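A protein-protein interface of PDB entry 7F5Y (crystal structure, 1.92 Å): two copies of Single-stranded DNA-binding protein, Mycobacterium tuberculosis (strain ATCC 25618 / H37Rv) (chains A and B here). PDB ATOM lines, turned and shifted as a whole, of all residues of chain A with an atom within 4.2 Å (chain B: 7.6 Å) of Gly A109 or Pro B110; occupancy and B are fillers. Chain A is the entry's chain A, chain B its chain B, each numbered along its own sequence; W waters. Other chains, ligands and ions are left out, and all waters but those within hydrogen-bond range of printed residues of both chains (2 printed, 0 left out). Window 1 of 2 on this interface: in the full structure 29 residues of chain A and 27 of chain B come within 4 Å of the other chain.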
ATOM      1  N   VAL A  79      -2.157   8.427  26.095  1.00  0.00           N
ATOM      2  CA  VAL A  79      -1.428   8.561  27.339  1.00  0.00           C
ATOM      3  C   VAL A  79      -1.371   7.229  28.081  1.00  0.00           C
ATOM      4  O   VAL A  79      -2.223   6.309  27.909  1.00  0.00           O
ATOM      5  CB  VAL A  79      -2.055   9.635  28.233  1.00  0.00           C
ATOM      6  CG1 VAL A  79      -1.999  10.992  27.576  1.00  0.00           C
ATOM      7  CG2 VAL A  79      -3.473   9.264  28.657  1.00  0.00           C
ATOM      8  N   ILE A  80      -0.347   7.116  28.930  1.00  0.00           N
ATOM      9  CA  ILE A  80      -0.246   6.069  29.916  1.00  0.00           C
ATOM     10  C   ILE A  80      -0.207   6.739  31.299  1.00  0.00           C
ATOM     11  O   ILE A  80       0.615   7.617  31.570  1.00  0.00           O
ATOM     12  CB  ILE A  80       0.948   5.124  29.655  1.00  0.00           C
ATOM     13  CG1 ILE A  80       1.243   4.252  30.878  1.00  0.00           C
ATOM     14  CG2 ILE A  80       2.179   5.890  29.215  1.00  0.00           C
ATOM     15  CD1 ILE A  80       2.195   3.111  30.604  1.00  0.00           C
ATOM     16  N   ILE A 108       1.996  10.324  34.597  1.00  0.00           N
ATOM     17  CA  ILE A 108       1.416  10.289  33.246  1.00  0.00           C
ATOM     18  C   ILE A 108       2.483  10.686  32.226  1.00  0.00           C
ATOM     19  O   ILE A 108       3.311  11.543  32.460  1.00  0.00           O
ATOM     20  CB  ILE A 108       0.166  11.182  33.123  1.00  0.00           C
ATOM     21  CG1 ILE A 108      -0.366  11.285  31.696  1.00  0.00           C
ATOM     22  CG2 ILE A 108       0.396  12.561  33.677  1.00  0.00           C
ATOM     23  CD1 ILE A 108      -1.709  11.973  31.648  1.00  0.00           C
ATOM     24  N   GLY A 109       2.411  10.051  31.062  1.00  0.00           N
ATOM     25  CA  GLY A 109       3.176  10.421  29.939  1.00  0.00           C
ATOM     26  C   GLY A 109       2.436  10.130  28.642  1.00  0.00           C
ATOM     27  O   GLY A 109       1.591   9.238  28.592  1.00  0.00           O
ATOM     28  N   PRO A 110       2.788  10.831  27.550  1.00  0.00           N
ATOM     29  CA  PRO A 110       2.289  10.496  26.218  1.00  0.00           C
ATOM     30  C   PRO A 110       2.953   9.196  25.773  1.00  0.00           C
ATOM     31  O   PRO A 110       4.142   9.079  25.912  1.00  0.00           O
ATOM     32  CB  PRO A 110       2.696  11.692  25.350  1.00  0.00           C
ATOM     33  CG  PRO A 110       3.941  12.251  26.069  1.00  0.00           C
ATOM     34  CD  PRO A 110       3.685  12.006  27.534  1.00  0.00           C
ATOM     35  N   SER A 111       2.146   8.241  25.288  1.00  0.00           N
ATOM     36  CA  SER A 111       2.642   6.992  24.713  1.00  0.00           C
ATOM     37  C   SER A 111       3.450   7.262  23.439  1.00  0.00           C
ATOM     38  O   SER A 111       3.083   8.146  22.663  1.00  0.00           O
ATOM     39  CB  SER A 111       1.522   6.055  24.368  1.00  0.00           C
ATOM     40  OG  SER A 111       2.096   4.861  23.865  1.00  0.00           O
ATOM     41  N   LEU A 112       4.509   6.461  23.227  1.00  0.00           N
ATOM     42  CA  LEU A 112       5.380   6.528  22.056  1.00  0.00           C
ATOM     43  C   LEU A 112       5.066   5.370  21.106  1.00  0.00           C
ATOM     44  O   LEU A 112       5.822   5.090  20.167  1.00  0.00           O
ATOM     45  CB  LEU A 112       6.842   6.511  22.502  1.00  0.00           C
ATOM     46  CG  LEU A 112       7.267   7.694  23.375  1.00  0.00           C
ATOM     47  CD1 LEU A 112       8.746   7.645  23.672  1.00  0.00           C
ATOM     48  CD2 LEU A 112       6.935   9.035  22.748  1.00  0.00           C
ATOM     49  N   VAL A 119      11.263  15.712  24.458  1.00  0.00           N
ATOM     50  CA  VAL A 119      11.142  15.783  25.915  1.00  0.00           C
ATOM     51  C   VAL A 119      12.105  16.857  26.422  1.00  0.00           C
ATOM     52  O   VAL A 119      13.231  16.918  25.971  1.00  0.00           O
ATOM     53  CB  VAL A 119      11.439  14.407  26.515  1.00  0.00           C
ATOM     54  CG1 VAL A 119      11.396  14.413  28.033  1.00  0.00           C
ATOM     55  CG2 VAL A 119      10.484  13.377  25.938  1.00  0.00           C
ATOM     56  N   SER B  72      13.233   9.368  20.723  1.00  0.00           N
ATOM     57  CA  SER B  72      12.606  10.320  21.649  1.00  0.00           C
ATOM     58  C   SER B  72      13.295  10.371  23.021  1.00  0.00           C
ATOM     59  O   SER B  72      13.201  11.390  23.745  1.00  0.00           O
ATOM     60  CB  SER B  72      11.161   9.958  21.826  1.00  0.00           C
ATOM     61  OG  SER B  72      10.447  10.035  20.597  1.00  0.00           O
ATOM     62  N   LEU B  73      13.877   9.252  23.445  1.00  0.00           N
ATOM     63  CA  LEU B  73      14.272   9.115  24.864  1.00  0.00           C
ATOM     64  C   LEU B  73      15.786   9.007  24.970  1.00  0.00           C
ATOM     65  O   LEU B  73      16.425   8.384  24.130  1.00  0.00           O
ATOM     66  CB  LEU B  73      13.621   7.864  25.432  1.00  0.00           C
ATOM     67  CG  LEU B  73      12.095   7.891  25.557  1.00  0.00           C
ATOM     68  CD1 LEU B  73      11.604   6.603  26.188  1.00  0.00           C
ATOM     69  CD2 LEU B  73      11.647   9.076  26.368  1.00  0.00           C
ATOM     70  N   ALA B  77      16.132   9.809  31.178  1.00  0.00           N
ATOM     71  CA  ALA B  77      14.746  10.202  31.019  1.00  0.00           C
ATOM     72  C   ALA B  77      13.869   9.411  32.005  1.00  0.00           C
ATOM     73  O   ALA B  77      14.010   8.173  32.168  1.00  0.00           O
ATOM     74  CB  ALA B  77      14.259   9.954  29.625  1.00  0.00           C
ATOM     75  N   ARG B  78      12.942  10.133  32.634  1.00  0.00           N
ATOM     76  CA  ARG B  78      11.939   9.524  33.488  1.00  0.00           C
ATOM     77  C   ARG B  78      10.814   8.971  32.599  1.00  0.00           C
ATOM     78  O   ARG B  78      10.190   9.708  31.836  1.00  0.00           O
ATOM     79  CB  ARG B  78      11.407  10.532  34.494  1.00  0.00           C
ATOM     80  CG  ARG B  78      10.573   9.878  35.585  1.00  0.00           C
ATOM     81  CD  ARG B  78      10.035  10.870  36.573  1.00  0.00           C
ATOM     82  NE  ARG B  78       9.173  10.242  37.554  1.00  0.00           N
ATOM     83  CZ  ARG B  78       9.619   9.615  38.645  1.00  0.00           C
ATOM     84  NH1 ARG B  78      10.913   9.567  38.894  1.00  0.00           N
ATOM     85  NH2 ARG B  78       8.770   9.078  39.497  1.00  0.00           N
ATOM     86  N   VAL B  79      10.576   7.667  32.710  1.00  0.00           N
ATOM     87  CA  VAL B  79       9.604   6.975  31.867  1.00  0.00           C
ATOM     88  C   VAL B  79       8.576   6.234  32.706  1.00  0.00           C
ATOM     89  O   VAL B  79       8.808   5.927  33.891  1.00  0.00           O
ATOM     90  CB  VAL B  79      10.288   6.001  30.913  1.00  0.00           C
ATOM     91  CG1 VAL B  79      11.198   6.762  29.975  1.00  0.00           C
ATOM     92  CG2 VAL B  79      11.060   4.894  31.641  1.00  0.00           C
ATOM     93  N   ILE B  80       7.440   5.953  32.071  1.00  0.00           N
ATOM     94  CA  ILE B  80       6.446   5.061  32.589  1.00  0.00           C
ATOM     95  C   ILE B  80       6.246   3.941  31.556  1.00  0.00           C
ATOM     96  O   ILE B  80       5.999   4.220  30.394  1.00  0.00           O
ATOM     97  CB  ILE B  80       5.149   5.813  32.953  1.00  0.00           C
ATOM     98  CG1 ILE B  80       4.020   4.823  33.269  1.00  0.00           C
ATOM     99  CG2 ILE B  80       4.771   6.805  31.866  1.00  0.00           C
ATOM    100  CD1 ILE B  80       2.813   5.439  33.959  1.00  0.00           C
ATOM    101  N   ILE B 108       5.227   2.690  26.434  1.00  0.00           N
ATOM    102  CA  ILE B 108       6.159   3.502  27.174  1.00  0.00           C
ATOM    103  C   ILE B 108       5.892   4.949  26.800  1.00  0.00           C
ATOM    104  O   ILE B 108       5.528   5.242  25.660  1.00  0.00           O
ATOM    105  CB  ILE B 108       7.623   3.082  26.919  1.00  0.00           C
ATOM    106  CG1 ILE B 108       8.620   4.018  27.605  1.00  0.00           C
ATOM    107  CG2 ILE B 108       7.897   2.926  25.428  1.00  0.00           C
ATOM    108  CD1 ILE B 108      10.028   3.500  27.636  1.00  0.00           C
ATOM    109  N   GLY B 109       6.074   5.849  27.779  1.00  0.00           N
ATOM    110  CA  GLY B 109       6.054   7.281  27.520  1.00  0.00           C
ATOM    111  C   GLY B 109       6.950   8.010  28.511  1.00  0.00           C
ATOM    112  O   GLY B 109       7.154   7.489  29.618  1.00  0.00           O
ATOM    113  N   PRO B 110       7.461   9.224  28.156  1.00  0.00           N
ATOM    114  CA  PRO B 110       8.220  10.057  29.087  1.00  0.00           C
ATOM    115  C   PRO B 110       7.211  10.566  30.122  1.00  0.00           C
ATOM    116  O   PRO B 110       6.156  11.056  29.752  1.00  0.00           O
ATOM    117  CB  PRO B 110       8.799  11.191  28.224  1.00  0.00           C
ATOM    118  CG  PRO B 110       7.875  11.273  27.035  1.00  0.00           C
ATOM    119  CD  PRO B 110       7.295   9.890  26.860  1.00  0.00           C
ATOM    120  N   SER B 111       7.563  10.449  31.410  1.00  0.00           N
ATOM    121  CA  SER B 111       6.744  11.074  32.480  1.00  0.00           C
ATOM    122  C   SER B 111       6.803  12.624  32.395  1.00  0.00           C
ATOM    123  O   SER B 111       7.860  13.232  32.201  1.00  0.00           O
ATOM    124  CB  SER B 111       7.177  10.572  33.829  1.00  0.00           C
ATOM    125  OG  SER B 111       6.610  11.334  34.879  1.00  0.00           O
ATOM    126  N   LEU B 112       5.665  13.248  32.672  1.00  0.00           N
ATOM    127  CA  LEU B 112       5.552  14.662  32.785  1.00  0.00           C
ATOM    128  C   LEU B 112       5.684  15.113  34.234  1.00  0.00           C
ATOM    129  O   LEU B 112       5.271  16.235  34.520  1.00  0.00           O
ATOM    130  CB  LEU B 112       4.200  15.098  32.229  1.00  0.00           C
ATOM    131  CG  LEU B 112       3.970  14.688  30.786  1.00  0.00           C
ATOM    132  CD1 LEU B 112       2.569  15.050  30.331  1.00  0.00           C
ATOM    133  CD2 LEU B 112       5.049  15.219  29.874  1.00  0.00           C
ATOM    134  N   ARG B 113       6.243  14.287  35.144  1.00  0.00           N
ATOM    135  CA  ARG B 113       6.392  14.742  36.511  1.00  0.00           C
ATOM    136  C   ARG B 113       7.337  15.947  36.583  1.00  0.00           C
ATOM    137  O   ARG B 113       7.024  16.944  37.254  1.00  0.00           O
ATOM    138  CB  ARG B 113       6.909  13.648  37.442  1.00  0.00           C
ATOM    139  CG  ARG B 113       7.152  14.134  38.861  1.00  0.00           C
ATOM    140  CD  ARG B 113       7.517  12.992  39.799  1.00  0.00           C
ATOM    141  NE  ARG B 113       6.337  12.246  40.167  1.00  0.00           N
ATOM    142  CZ  ARG B 113       6.169  11.622  41.322  1.00  0.00           C
ATOM    143  NH1 ARG B 113       5.219  10.710  41.434  1.00  0.00           N
ATOM    144  NH2 ARG B 113       6.974  11.876  42.333  1.00  0.00           N
ATOM    145  N   ALA B 115       8.991  17.160  33.540  1.00  0.00           N
ATOM    146  CA  ALA B 115       9.319  17.524  32.186  1.00  0.00           C
ATOM    147  C   ALA B 115       8.044  17.813  31.396  1.00  0.00           C
ATOM    148  O   ALA B 115       6.926  17.455  31.813  1.00  0.00           O
ATOM    149  CB  ALA B 115      10.142  16.440  31.503  1.00  0.00           C
ATOM    150  N   THR B 116       8.238  18.519  30.270  1.00  0.00           N
ATOM    151  CA  THR B 116       7.236  18.679  29.292  1.00  0.00           C
ATOM    152  C   THR B 116       7.667  17.827  28.106  1.00  0.00           C
ATOM    153  O   THR B 116       8.818  17.439  27.950  1.00  0.00           O
ATOM    154  CB  THR B 116       7.026  20.150  28.874  1.00  0.00           C
ATOM    155  OG1 THR B 116       8.264  20.627  28.343  1.00  0.00           O
ATOM    156  CG2 THR B 116       6.602  21.034  30.013  1.00  0.00           C
ATOM    157  N   ALA B 117       6.709  17.575  27.238  1.00  0.00           N
ATOM    158  CA  ALA B 117       6.969  16.930  26.004  1.00  0.00           C
ATOM    159  C   ALA B 117       6.126  17.646  24.952  1.00  0.00           C
ATOM    160  O   ALA B 117       5.061  18.170  25.270  1.00  0.00           O
ATOM    161  CB  ALA B 117       6.655  15.459  26.114  1.00  0.00           C
ATOM    162  N   LYS B 118       6.673  17.709  23.740  1.00  0.00           N
ATOM    163  CA  LYS B 118       5.975  18.047  22.526  1.00  0.00           C
ATOM    164  C   LYS B 118       5.782  16.726  21.769  1.00  0.00           C
ATOM    165  O   LYS B 118       6.734  16.147  21.326  1.00  0.00           O
ATOM    166  CB  LYS B 118       6.818  19.097  21.780  1.00  0.00           C
ATOM    167  CG  LYS B 118       6.184  19.783  20.574  1.00  0.00           C
ATOM    168  N   VAL B 119       4.538  16.254  21.688  1.00  0.00           N
ATOM    169  CA  VAL B 119       4.165  15.044  21.035  1.00  0.00           C
ATOM    170  C   VAL B 119       4.074  15.305  19.527  1.00  0.00           C
ATOM    171  O   VAL B 119       3.383  16.226  19.106  1.00  0.00           O
ATOM    172  CB  VAL B 119       2.808  14.547  21.563  1.00  0.00           C
ATOM    173  CG1 VAL B 119       2.400  13.247  20.901  1.00  0.00           C
ATOM    174  CG2 VAL B 119       2.803  14.416  23.079  1.00  0.00           C
HETATM  175  O   HOH W   1      12.944  13.923  23.224  1.00  0.00           O
HETATM  176  O   HOH W   2       3.652  12.384  35.576  1.00  0.00           O
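The backbone carbonyl oxygen (O) of Gly B109 lies within hydrogen-bond range of the backbone NH (N) of Ile B80 (2.9 Å).
OG of Ser B111 sits at hydrogen-bond distance from N of Arg B113 (3.0 Å).
The backbone NH (N) of Ser B111 sits at hydrogen-bond distance from the backbone carbonyl oxygen (O) of Arg B78.
The backbone carbonyl oxygen of Gly A109 sits at hydrogen-bond distance from the backbone NH of Ile A80, 2.9 Å away.
O of Ile B108 is in hydrogen-bond range of N of Leu A112.
O of Ile A108 is in hydrogen-bond range of N of Leu B112 (2.9 Å).
Hydrophobic or aromatic side chains of chain A within 4 Å of the printed part of chain B: Ile A80, Pro A110, Leu A112 and Val A119.
Hydrophobic or aromatic side chains of chain B within 4 Å of the printed part of chain A: Leu B73, Ile B80, Pro B110, Leu B112 and Val B119.
Among the printed residues, 14 pairs touch across the chains.
Among the printed residues, no Asp or Glu carboxylate lies within 4 Å of a Lys or Arg side-chain nitrogen of the other chain.
Ile A80 touches its own counterpart, Ile B80.
Ile A108 touches Pro B110, but with the chains exchanged Pro A110 does not touch Ile B108 (4.1 Å).
Ile A108 touches Ser B111, and with the chains exchanged Ser A111 touches Ile B108.
Gly A109 touches Pro B110, and with the chains exchanged Pro A110 touches Gly B109.
8 positions are printed for both chains.
Among the printed residues, pairs that only touch across the chains: Gly A109 with Pro B110 (3.1 Å), Pro A110 with Gly B109 (3.1 Å), Pro A110 with Pro B110 (3.4 Å), Ile A108 with Ser B111 (3.5 Å), Val A119 with Thr B116 (3.5 Å), Ser A111 with Ile B108 (3.5 Å), Val A119 with Pro B110 (3.5 Å), Pro A110 with Val B119 (3.5 Å), Ile A80 with Ile B80 (3.7 Å), Leu A112 with Ser B72 (3.8 Å), Leu A112 with Leu B73 (3.9 Å) and Ile A108 with Pro B110 (3.96 Å).
Of the printed residues of chain B, Gly A109 touches Pro B110 (3.1 Å).
Pro B110 touches just these residues of chain A: Ile A108, Gly A109, Pro A110 and Val A119.
Of the printed residues of chain B, Ile A108 touches Pro B110, Ser B111 and Leu B112.
Printed residues of chain B within 4 Å of Leu A112: Ser B72 (3.8 Å), Leu B73 (3.9 Å) and Ile B108 (2.9 Å).
Of the printed residues of chain B, Ser A111 touches Ile B108 (3.5 Å).
Of the printed residues of chain A, Gly B109 touches Pro A110 (3.1 Å).
Ala B117 touches none of the printed residues of chain A.
Arg B113 touches none of the printed residues of chain A.
The nearest printed residue of chain B that does not touch Gly A109 is Ile B80 (4.1 Å).
The nearest printed residue of chain A that does not touch Val B119 is Ser A111 (5.4 Å).
Water W1 bridges the backbone carbonyl oxygen (O) of Ser B72 (2.6 Å) and the backbone NH (N) of Val A119 (2.7 Å).
Water W2 lies within hydrogen-bond range of the backbone NH (N) of Ile A108, the side-chain hydroxyl (OG) of Ser B111 and the backbone NH (N) of Arg B113.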
